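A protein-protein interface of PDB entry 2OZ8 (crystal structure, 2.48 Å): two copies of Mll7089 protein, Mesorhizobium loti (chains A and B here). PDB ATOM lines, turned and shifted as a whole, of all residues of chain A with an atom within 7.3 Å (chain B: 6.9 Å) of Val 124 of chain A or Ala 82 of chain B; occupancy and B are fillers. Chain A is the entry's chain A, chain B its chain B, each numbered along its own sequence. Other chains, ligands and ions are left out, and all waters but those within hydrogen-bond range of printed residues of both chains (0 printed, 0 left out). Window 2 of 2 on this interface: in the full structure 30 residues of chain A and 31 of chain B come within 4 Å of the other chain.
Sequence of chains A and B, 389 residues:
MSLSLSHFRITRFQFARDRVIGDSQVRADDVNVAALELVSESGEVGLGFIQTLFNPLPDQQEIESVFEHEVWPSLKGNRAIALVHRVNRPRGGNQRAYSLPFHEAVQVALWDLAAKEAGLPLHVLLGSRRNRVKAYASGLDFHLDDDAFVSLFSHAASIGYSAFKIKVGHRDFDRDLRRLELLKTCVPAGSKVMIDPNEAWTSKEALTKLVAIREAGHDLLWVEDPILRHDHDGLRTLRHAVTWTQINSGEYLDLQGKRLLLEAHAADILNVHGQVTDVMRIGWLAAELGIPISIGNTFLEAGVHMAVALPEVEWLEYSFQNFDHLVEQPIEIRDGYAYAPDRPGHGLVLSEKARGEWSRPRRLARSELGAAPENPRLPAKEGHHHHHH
ND1 of His 85 of chain B is in hydrogen-bond range of O of Leu 125 of chain A (2.9 Å).
The guanidinium group (NE) of Arg 86 of chain B lies within hydrogen-bond range of the backbone carbonyl oxygen (O) of Gly 127 of chain A.
The backbone carbonyl oxygen (O) of Ser 128 of chain A sits at hydrogen-bond distance from the guanidinium group (NH2) of Arg 86 of chain B, 3.3 Å away.
The backbone carbonyl oxygen of Leu 126 of chain A sits close to the backbone carbonyl oxygen of His 85 of chain B (3.4 Å).
The backbone NH (N) of Gly 345 of chain A lies within hydrogen-bond range of the backbone carbonyl oxygen (O) of Leu 120 of chain A, 3.0 Å away.
ND1 of His 123 of chain A is in hydrogen-bond range of OG of Ser 128 of chain A (2.6 Å).
The side-chain hydroxyl of Ser 128 of chain A sits at hydrogen-bond distance from the backbone carbonyl oxygen of Arg 130 of chain A (3.2 Å).
A ring nitrogen (ND1) of His 85 of chain B is in hydrogen-bond range of the backbone carbonyl oxygen (O) of Ile 81 of chain B (2.8 Å).
Among the printed residues, pairs that only touch across the chains: Leu 120 of chain A with Arg 79 of chain B (3.7 Å), Leu 120 of chain A with Ile 81 of chain B (3.97 Å), Val 124 of chain A with Ala 82 of chain B (3.2 Å), Leu 125 of chain A with Ile 81 of chain B (3.6 Å), Leu 125 of chain A with Ala 82 of chain B (3.8 Å), Gly 127 of chain A with Ala 82 of chain B (3.5 Å) and Arg 129 of chain A with Arg 86 of chain B (3.6 Å).
Of the printed residues of chain B, Leu 120 of chain A touches Arg 79 and Ile 81.
Val 124 of chain A touches one residue of chain B.
Of the printed residues of chain B, Leu 125 of chain A touches Ile 81 (3.6 Å), Ala 82 (3.8 Å) and His 85 (2.9 Å).
Ala 82 of chain B touches just these residues of chain A: Val 124, Leu 125 and Gly 127.
Of the printed residues of chain A, His 85 of chain B touches Leu 125 (2.9 Å) and Leu 126 (3.4 Å).
Printed residues of chain A within 4 Å of Arg 86 of chain B: Gly 127 (2.8 Å), Ser 128 (3.3 Å) and Arg 129 (3.6 Å).
Printed residues of chain B that touch a printed residue of chain A: Arg 79, Ile 81, Ala 82, His 85 and Arg 86.
Along chain B the printed residues that touch a printed residue of chain A span positions 79 to 86.
Among the printed residues, 11 pairs touch across the chains.
No position is printed for both chains.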
ATOM      1  N   LEU A 120      16.009 -13.829   0.455  1.00  0.00           N
ATOM      2  CA  LEU A 120      14.809 -14.627   0.280  1.00  0.00           C
ATOM      3  C   LEU A 120      14.886 -15.920   1.076  1.00  0.00           C
ATOM      4  O   LEU A 120      15.997 -16.462   1.290  1.00  0.00           O
ATOM      5  CB  LEU A 120      14.560 -14.979  -1.206  1.00  0.00           C
ATOM      6  CG  LEU A 120      14.244 -13.884  -2.249  1.00  0.00           C
ATOM      7  CD1 LEU A 120      14.335 -14.430  -3.709  1.00  0.00           C
ATOM      8  CD2 LEU A 120      12.884 -13.259  -1.995  1.00  0.00           C
ATOM      9  N   PRO A 121      13.698 -16.430   1.479  1.00  0.00           N
ATOM     10  CA  PRO A 121      13.527 -17.824   1.917  1.00  0.00           C
ATOM     11  C   PRO A 121      13.815 -18.756   0.745  1.00  0.00           C
ATOM     12  O   PRO A 121      13.425 -18.453  -0.389  1.00  0.00           O
ATOM     13  CB  PRO A 121      12.044 -17.913   2.286  1.00  0.00           C
ATOM     14  CG  PRO A 121      11.497 -16.445   2.307  1.00  0.00           C
ATOM     15  CD  PRO A 121      12.420 -15.675   1.439  1.00  0.00           C
ATOM     16  N   LEU A 122      14.488 -19.872   1.005  1.00  0.00           N
ATOM     17  CA  LEU A 122      14.846 -20.813  -0.085  1.00  0.00           C
ATOM     18  C   LEU A 122      13.703 -21.229  -1.046  1.00  0.00           C
ATOM     19  O   LEU A 122      13.851 -21.124  -2.269  1.00  0.00           O
ATOM     20  CB  LEU A 122      15.624 -22.018   0.451  1.00  0.00           C
ATOM     21  CG  LEU A 122      16.096 -23.023  -0.602  1.00  0.00           C
ATOM     22  CD1 LEU A 122      17.060 -22.387  -1.653  1.00  0.00           C
ATOM     23  CD2 LEU A 122      16.737 -24.170   0.086  1.00  0.00           C
ATOM     24  N   HIS A 123      12.563 -21.643  -0.509  1.00  0.00           N
ATOM     25  CA  HIS A 123      11.423 -22.029  -1.334  1.00  0.00           C
ATOM     26  C   HIS A 123      10.920 -20.963  -2.323  1.00  0.00           C
ATOM     27  O   HIS A 123      10.548 -21.292  -3.468  1.00  0.00           O
ATOM     28  CB  HIS A 123      10.275 -22.583  -0.474  1.00  0.00           C
ATOM     29  CG  HIS A 123       9.562 -21.564   0.348  1.00  0.00           C
ATOM     30  ND1 HIS A 123       8.343 -21.018  -0.026  1.00  0.00           N
ATOM     31  CD2 HIS A 123       9.871 -21.008   1.549  1.00  0.00           C
ATOM     32  CE1 HIS A 123       7.934 -20.178   0.911  1.00  0.00           C
ATOM     33  NE2 HIS A 123       8.845 -20.149   1.872  1.00  0.00           N
ATOM     34  N   VAL A 124      10.890 -19.706  -1.888  1.00  0.00           N
ATOM     35  CA  VAL A 124      10.489 -18.604  -2.783  1.00  0.00           C
ATOM     36  C   VAL A 124      11.508 -18.492  -3.939  1.00  0.00           C
ATOM     37  O   VAL A 124      11.131 -18.432  -5.104  1.00  0.00           O
ATOM     38  CB  VAL A 124      10.336 -17.241  -2.020  1.00  0.00           C
ATOM     39  CG1 VAL A 124       9.999 -16.110  -2.997  1.00  0.00           C
ATOM     40  CG2 VAL A 124       9.277 -17.355  -0.860  1.00  0.00           C
ATOM     41  N   LEU A 125      12.791 -18.509  -3.600  1.00  0.00           N
ATOM     42  CA  LEU A 125      13.849 -18.579  -4.615  1.00  0.00           C
ATOM     43  C   LEU A 125      13.645 -19.818  -5.530  1.00  0.00           C
ATOM     44  O   LEU A 125      13.922 -19.751  -6.745  1.00  0.00           O
ATOM     45  CB  LEU A 125      15.237 -18.619  -3.960  1.00  0.00           C
ATOM     46  CG  LEU A 125      16.452 -18.706  -4.886  1.00  0.00           C
ATOM     47  CD1 LEU A 125      16.686 -17.412  -5.783  1.00  0.00           C
ATOM     48  CD2 LEU A 125      17.717 -19.039  -4.039  1.00  0.00           C
ATOM     49  N   LEU A 126      13.151 -20.920  -4.948  1.00  0.00           N
ATOM     50  CA  LEU A 126      12.919 -22.158  -5.745  1.00  0.00           C
ATOM     51  C   LEU A 126      11.678 -22.070  -6.633  1.00  0.00           C
ATOM     52  O   LEU A 126      11.406 -23.001  -7.383  1.00  0.00           O
ATOM     53  CB  LEU A 126      12.940 -23.446  -4.897  1.00  0.00           C
ATOM     54  CG  LEU A 126      14.306 -23.742  -4.235  1.00  0.00           C
ATOM     55  CD1 LEU A 126      14.239 -24.956  -3.346  1.00  0.00           C
ATOM     56  CD2 LEU A 126      15.473 -23.792  -5.274  1.00  0.00           C
ATOM     57  N   GLY A 127      10.993 -20.918  -6.578  1.00  0.00           N
ATOM     58  CA  GLY A 127       9.795 -20.644  -7.364  1.00  0.00           C
ATOM     59  C   GLY A 127       8.485 -21.079  -6.705  1.00  0.00           C
ATOM     60  O   GLY A 127       7.472 -21.149  -7.372  1.00  0.00           O
ATOM     61  N   SER A 128       8.464 -21.338  -5.401  1.00  0.00           N
ATOM     62  CA  SER A 128       7.247 -21.854  -4.797  1.00  0.00           C
ATOM     63  C   SER A 128       6.107 -20.883  -4.950  1.00  0.00           C
ATOM     64  O   SER A 128       6.325 -19.682  -5.142  1.00  0.00           O
ATOM     65  CB  SER A 128       7.430 -22.195  -3.308  1.00  0.00           C
ATOM     66  OG  SER A 128       7.467 -21.009  -2.507  1.00  0.00           O
ATOM     67  N   ARG A 129       4.891 -21.424  -4.857  1.00  0.00           N
ATOM     68  CA  ARG A 129       3.659 -20.638  -4.798  1.00  0.00           C
ATOM     69  C   ARG A 129       2.961 -20.985  -3.491  1.00  0.00           C
ATOM     70  O   ARG A 129       1.966 -20.381  -3.136  1.00  0.00           O
ATOM     71  CB  ARG A 129       2.711 -20.988  -5.932  1.00  0.00           C
ATOM     72  CG  ARG A 129       3.300 -20.938  -7.322  1.00  0.00           C
ATOM     73  CD  ARG A 129       2.200 -20.568  -8.345  1.00  0.00           C
ATOM     74  NE  ARG A 129       2.461 -21.239  -9.606  1.00  0.00           N
ATOM     75  CZ  ARG A 129       2.109 -20.755 -10.784  1.00  0.00           C
ATOM     76  NH1 ARG A 129       1.455 -19.600 -10.856  1.00  0.00           N
ATOM     77  NH2 ARG A 129       2.431 -21.410 -11.891  1.00  0.00           N
ATOM     78  N   ARG A 130       3.459 -21.989  -2.791  1.00  0.00           N
ATOM     79  CA  ARG A 130       2.885 -22.321  -1.519  1.00  0.00           C
ATOM     80  C   ARG A 130       3.958 -22.435  -0.465  1.00  0.00           C
ATOM     81  O   ARG A 130       5.142 -22.360  -0.755  1.00  0.00           O
ATOM     82  CB  ARG A 130       1.963 -23.555  -1.608  1.00  0.00           C
ATOM     83  CG  ARG A 130       2.590 -24.896  -2.127  1.00  0.00           C
ATOM     84  CD  ARG A 130       1.469 -25.860  -2.695  1.00  0.00           C
ATOM     85  NE  ARG A 130       0.748 -25.171  -3.789  1.00  0.00           N
ATOM     86  CZ  ARG A 130      -0.572 -25.213  -4.002  1.00  0.00           C
ATOM     87  NH1 ARG A 130      -1.359 -25.938  -3.212  1.00  0.00           N
ATOM     88  NH2 ARG A 130      -1.099 -24.519  -5.013  1.00  0.00           N
ATOM     89  N   ASN A 131       3.541 -22.573   0.775  1.00  0.00           N
ATOM     90  CA  ASN A 131       4.493 -22.605   1.836  1.00  0.00           C
ATOM     91  C   ASN A 131       4.350 -23.836   2.713  1.00  0.00           C
ATOM     92  O   ASN A 131       4.988 -23.930   3.753  1.00  0.00           O
ATOM     93  CB  ASN A 131       4.501 -21.265   2.609  1.00  0.00           C
ATOM     94  CG  ASN A 131       3.534 -21.232   3.764  1.00  0.00           C
ATOM     95  OD1 ASN A 131       2.399 -21.723   3.670  1.00  0.00           O
ATOM     96  ND2 ASN A 131       3.986 -20.655   4.897  1.00  0.00           N
ATOM     97  N   HIS A 305      11.764 -27.095   1.446  1.00  0.00           N
ATOM     98  CA  HIS A 305      11.732 -26.040   0.467  1.00  0.00           C
ATOM     99  C   HIS A 305      11.524 -26.534  -0.949  1.00  0.00           C
ATOM    100  O   HIS A 305      10.798 -25.895  -1.708  1.00  0.00           O
ATOM    101  CB  HIS A 305      12.986 -25.214   0.591  1.00  0.00           C
ATOM    102  CG  HIS A 305      13.070 -24.494   1.897  1.00  0.00           C
ATOM    103  ND1 HIS A 305      12.483 -23.267   2.102  1.00  0.00           N
ATOM    104  CD2 HIS A 305      13.657 -24.840   3.070  1.00  0.00           C
ATOM    105  CE1 HIS A 305      12.698 -22.892   3.349  1.00  0.00           C
ATOM    106  NE2 HIS A 305      13.414 -23.823   3.952  1.00  0.00           N
ATOM    107  N   VAL A 308       7.744 -27.969  -1.058  1.00  0.00           N
ATOM    108  CA  VAL A 308       6.702 -26.992  -1.322  1.00  0.00           C
ATOM    109  C   VAL A 308       6.927 -26.362  -2.681  1.00  0.00           C
ATOM    110  O   VAL A 308       5.975 -25.863  -3.236  1.00  0.00           O
ATOM    111  CB  VAL A 308       6.509 -25.838  -0.207  1.00  0.00           C
ATOM    112  CG1 VAL A 308       6.522 -26.362   1.212  1.00  0.00           C
ATOM    113  CG2 VAL A 308       7.512 -24.712  -0.358  1.00  0.00           C
ATOM    114  N   ALA A 309       8.153 -26.357  -3.230  1.00  0.00           N
ATOM    115  CA  ALA A 309       8.339 -25.650  -4.501  1.00  0.00           C
ATOM    116  C   ALA A 309       8.020 -26.476  -5.762  1.00  0.00           C
ATOM    117  O   ALA A 309       7.650 -25.923  -6.799  1.00  0.00           O
ATOM    118  CB  ALA A 309       9.721 -24.984  -4.590  1.00  0.00           C
ATOM    119  N   ALA A 340       7.417 -24.482   5.213  1.00  0.00           N
ATOM    120  CA  ALA A 340       8.646 -23.814   4.836  1.00  0.00           C
ATOM    121  C   ALA A 340       8.580 -22.397   5.395  1.00  0.00           C
ATOM    122  O   ALA A 340       7.668 -21.630   5.037  1.00  0.00           O
ATOM    123  CB  ALA A 340       8.798 -23.790   3.344  1.00  0.00           C
ATOM    124  N   PRO A 341       9.532 -22.038   6.277  1.00  0.00           N
ATOM    125  CA  PRO A 341       9.522 -20.772   7.017  1.00  0.00           C
ATOM    126  C   PRO A 341       9.789 -19.550   6.164  1.00  0.00           C
ATOM    127  O   PRO A 341      10.366 -19.659   5.071  1.00  0.00           O
ATOM    128  CB  PRO A 341      10.664 -20.933   8.019  1.00  0.00           C
ATOM    129  CG  PRO A 341      11.529 -21.969   7.471  1.00  0.00           C
ATOM    130  CD  PRO A 341      10.720 -22.856   6.590  1.00  0.00           C
ATOM    131  N   ASP A 342       9.409 -18.383   6.686  1.00  0.00           N
ATOM    132  CA  ASP A 342       9.587 -17.104   5.993  1.00  0.00           C
ATOM    133  C   ASP A 342      10.890 -16.392   6.363  1.00  0.00           C
ATOM    134  O   ASP A 342      11.006 -15.193   6.200  1.00  0.00           O
ATOM    135  CB  ASP A 342       8.371 -16.192   6.211  1.00  0.00           C
ATOM    136  CG  ASP A 342       8.430 -14.907   5.374  1.00  0.00           C
ATOM    137  OD1 ASP A 342       8.879 -14.972   4.209  1.00  0.00           O
ATOM    138  OD2 ASP A 342       8.042 -13.826   5.888  1.00  0.00           O
ATOM    139  N   GLY A 345      17.282 -17.968   3.542  1.00  0.00           N
ATOM    140  CA  GLY A 345      17.863 -19.285   3.435  1.00  0.00           C
ATOM    141  C   GLY A 345      16.824 -20.371   3.635  1.00  0.00           C
ATOM    142  O   GLY A 345      15.599 -20.183   3.373  1.00  0.00           O
ATOM    143  N   ASN B  78       6.254 -10.135  -8.117  1.00  0.00           N
ATOM    144  CA  ASN B  78       7.257 -11.203  -7.951  1.00  0.00           C
ATOM    145  C   ASN B  78       8.725 -10.804  -8.214  1.00  0.00           C
ATOM    146  O   ASN B  78       8.982  -9.836  -8.905  1.00  0.00           O
ATOM    147  CB  ASN B  78       6.865 -12.420  -8.817  1.00  0.00           C
ATOM    148  CG  ASN B  78       5.491 -12.982  -8.442  1.00  0.00           C
ATOM    149  OD1 ASN B  78       5.300 -13.424  -7.320  1.00  0.00           O
ATOM    150  ND2 ASN B  78       4.539 -12.976  -9.386  1.00  0.00           N
ATOM    151  N   ARG B  79       9.667 -11.571  -7.647  1.00  0.00           N
ATOM    152  CA  ARG B  79      11.100 -11.430  -7.921  1.00  0.00           C
ATOM    153  C   ARG B  79      11.492 -12.228  -9.150  1.00  0.00           C
ATOM    154  O   ARG B  79      11.148 -13.431  -9.247  1.00  0.00           O
ATOM    155  CB  ARG B  79      11.922 -11.959  -6.754  1.00  0.00           C
ATOM    156  CG  ARG B  79      11.855 -11.120  -5.494  1.00  0.00           C
ATOM    157  CD  ARG B  79      12.762  -9.894  -5.545  1.00  0.00           C
ATOM    158  NE  ARG B  79      14.157 -10.172  -5.923  1.00  0.00           N
ATOM    159  CZ  ARG B  79      15.107 -10.480  -5.052  1.00  0.00           C
ATOM    160  NH1 ARG B  79      14.807 -10.585  -3.755  1.00  0.00           N
ATOM    161  NH2 ARG B  79      16.347 -10.660  -5.465  1.00  0.00           N
ATOM    162  N   ALA B  80      12.210 -11.575 -10.076  1.00  0.00           N
ATOM    163  CA  ALA B  80      12.738 -12.234 -11.272  1.00  0.00           C
ATOM    164  C   ALA B  80      13.490 -13.520 -10.968  1.00  0.00           C
ATOM    165  O   ALA B  80      13.272 -14.533 -11.624  1.00  0.00           O
ATOM    166  CB  ALA B  80      13.674 -11.289 -12.061  1.00  0.00           C
ATOM    167  N   ILE B  81      14.417 -13.451 -10.010  1.00  0.00           N
ATOM    168  CA  ILE B  81      15.242 -14.608  -9.666  1.00  0.00           C
ATOM    169  C   ILE B  81      14.380 -15.759  -9.120  1.00  0.00           C
ATOM    170  O   ILE B  81      14.753 -16.902  -9.268  1.00  0.00           O
ATOM    171  CB  ILE B  81      16.449 -14.224  -8.721  1.00  0.00           C
ATOM    172  CG1 ILE B  81      17.518 -15.336  -8.638  1.00  0.00           C
ATOM    173  CG2 ILE B  81      15.970 -13.888  -7.289  1.00  0.00           C
ATOM    174  CD1 ILE B  81      18.198 -15.763  -9.929  1.00  0.00           C
ATOM    175  N   ALA B  82      13.226 -15.458  -8.517  1.00  0.00           N
ATOM    176  CA  ALA B  82      12.275 -16.483  -8.044  1.00  0.00           C
ATOM    177  C   ALA B  82      11.555 -17.110  -9.207  1.00  0.00           C
ATOM    178  O   ALA B  82      11.503 -18.322  -9.318  1.00  0.00           O
ATOM    179  CB  ALA B  82      11.232 -15.907  -6.997  1.00  0.00           C
ATOM    180  N   LEU B  83      10.981 -16.286 -10.069  1.00  0.00           N
ATOM    181  CA  LEU B  83      10.248 -16.780 -11.225  1.00  0.00           C
ATOM    182  C   LEU B  83      11.017 -17.735 -12.140  1.00  0.00           C
ATOM    183  O   LEU B  83      10.428 -18.656 -12.687  1.00  0.00           O
ATOM    184  CB  LEU B  83       9.745 -15.609 -12.052  1.00  0.00           C
ATOM    185  CG  LEU B  83       8.642 -14.822 -11.328  1.00  0.00           C
ATOM    186  CD1 LEU B  83       8.428 -13.420 -11.953  1.00  0.00           C
ATOM    187  CD2 LEU B  83       7.335 -15.614 -11.239  1.00  0.00           C
ATOM    188  N   VAL B  84      12.316 -17.495 -12.338  1.00  0.00           N
ATOM    189  CA  VAL B  84      13.068 -18.280 -13.313  1.00  0.00           C
ATOM    190  C   VAL B  84      13.308 -19.741 -12.864  1.00  0.00           C
ATOM    191  O   VAL B  84      13.670 -20.590 -13.703  1.00  0.00           O
ATOM    192  CB  VAL B  84      14.450 -17.615 -13.721  1.00  0.00           C
ATOM    193  CG1 VAL B  84      14.216 -16.327 -14.520  1.00  0.00           C
ATOM    194  CG2 VAL B  84      15.426 -17.468 -12.497  1.00  0.00           C
ATOM    195  N   HIS B  85      13.159 -20.011 -11.569  1.00  0.00           N
ATOM    196  CA  HIS B  85      13.451 -21.360 -11.036  1.00  0.00           C
ATOM    197  C   HIS B  85      12.183 -22.191 -10.999  1.00  0.00           C
ATOM    198  O   HIS B  85      12.236 -23.364 -10.710  1.00  0.00           O
ATOM    199  CB  HIS B  85      14.085 -21.315  -9.635  1.00  0.00           C
ATOM    200  CG  HIS B  85      15.456 -20.702  -9.602  1.00  0.00           C
ATOM    201  ND1 HIS B  85      15.717 -19.487  -9.004  1.00  0.00           N
ATOM    202  CD2 HIS B  85      16.646 -21.141 -10.080  1.00  0.00           C
ATOM    203  CE1 HIS B  85      17.008 -19.205  -9.120  1.00  0.00           C
ATOM    204  NE2 HIS B  85      17.592 -20.188  -9.779  1.00  0.00           N
ATOM    205  N   ARG B  86      11.039 -21.571 -11.292  1.00  0.00           N
ATOM    206  CA  ARG B  86       9.757 -22.258 -11.200  1.00  0.00           C
ATOM    207  C   ARG B  86       9.661 -23.433 -12.118  1.00  0.00           C
ATOM    208  O   ARG B  86       9.998 -23.348 -13.291  1.00  0.00           O
ATOM    209  CB  ARG B  86       8.599 -21.348 -11.496  1.00  0.00           C
ATOM    210  CG  ARG B  86       7.250 -22.009 -11.218  1.00  0.00           C
ATOM    211  CD  ARG B  86       6.152 -20.966 -11.047  1.00  0.00           C
ATOM    212  NE  ARG B  86       6.330 -20.235  -9.801  1.00  0.00           N
ATOM    213  CZ  ARG B  86       5.724 -19.089  -9.474  1.00  0.00           C
ATOM    214  NH1 ARG B  86       4.877 -18.492 -10.344  1.00  0.00           N
ATOM    215  NH2 ARG B  86       5.958 -18.572  -8.253  1.00  0.00           N
ATOM    216  N   ALA B 114      17.109 -10.740 -13.228  1.00  0.00           N
ATOM    217  CA  ALA B 114      17.699 -11.489 -12.144  1.00  0.00           C
ATOM    218  C   ALA B 114      19.206 -11.259 -12.028  1.00  0.00           C
ATOM    219  O   ALA B 114      19.732 -11.090 -10.911  1.00  0.00           O
ATOM    220  CB  ALA B 114      17.403 -12.982 -12.319  1.00  0.00           C
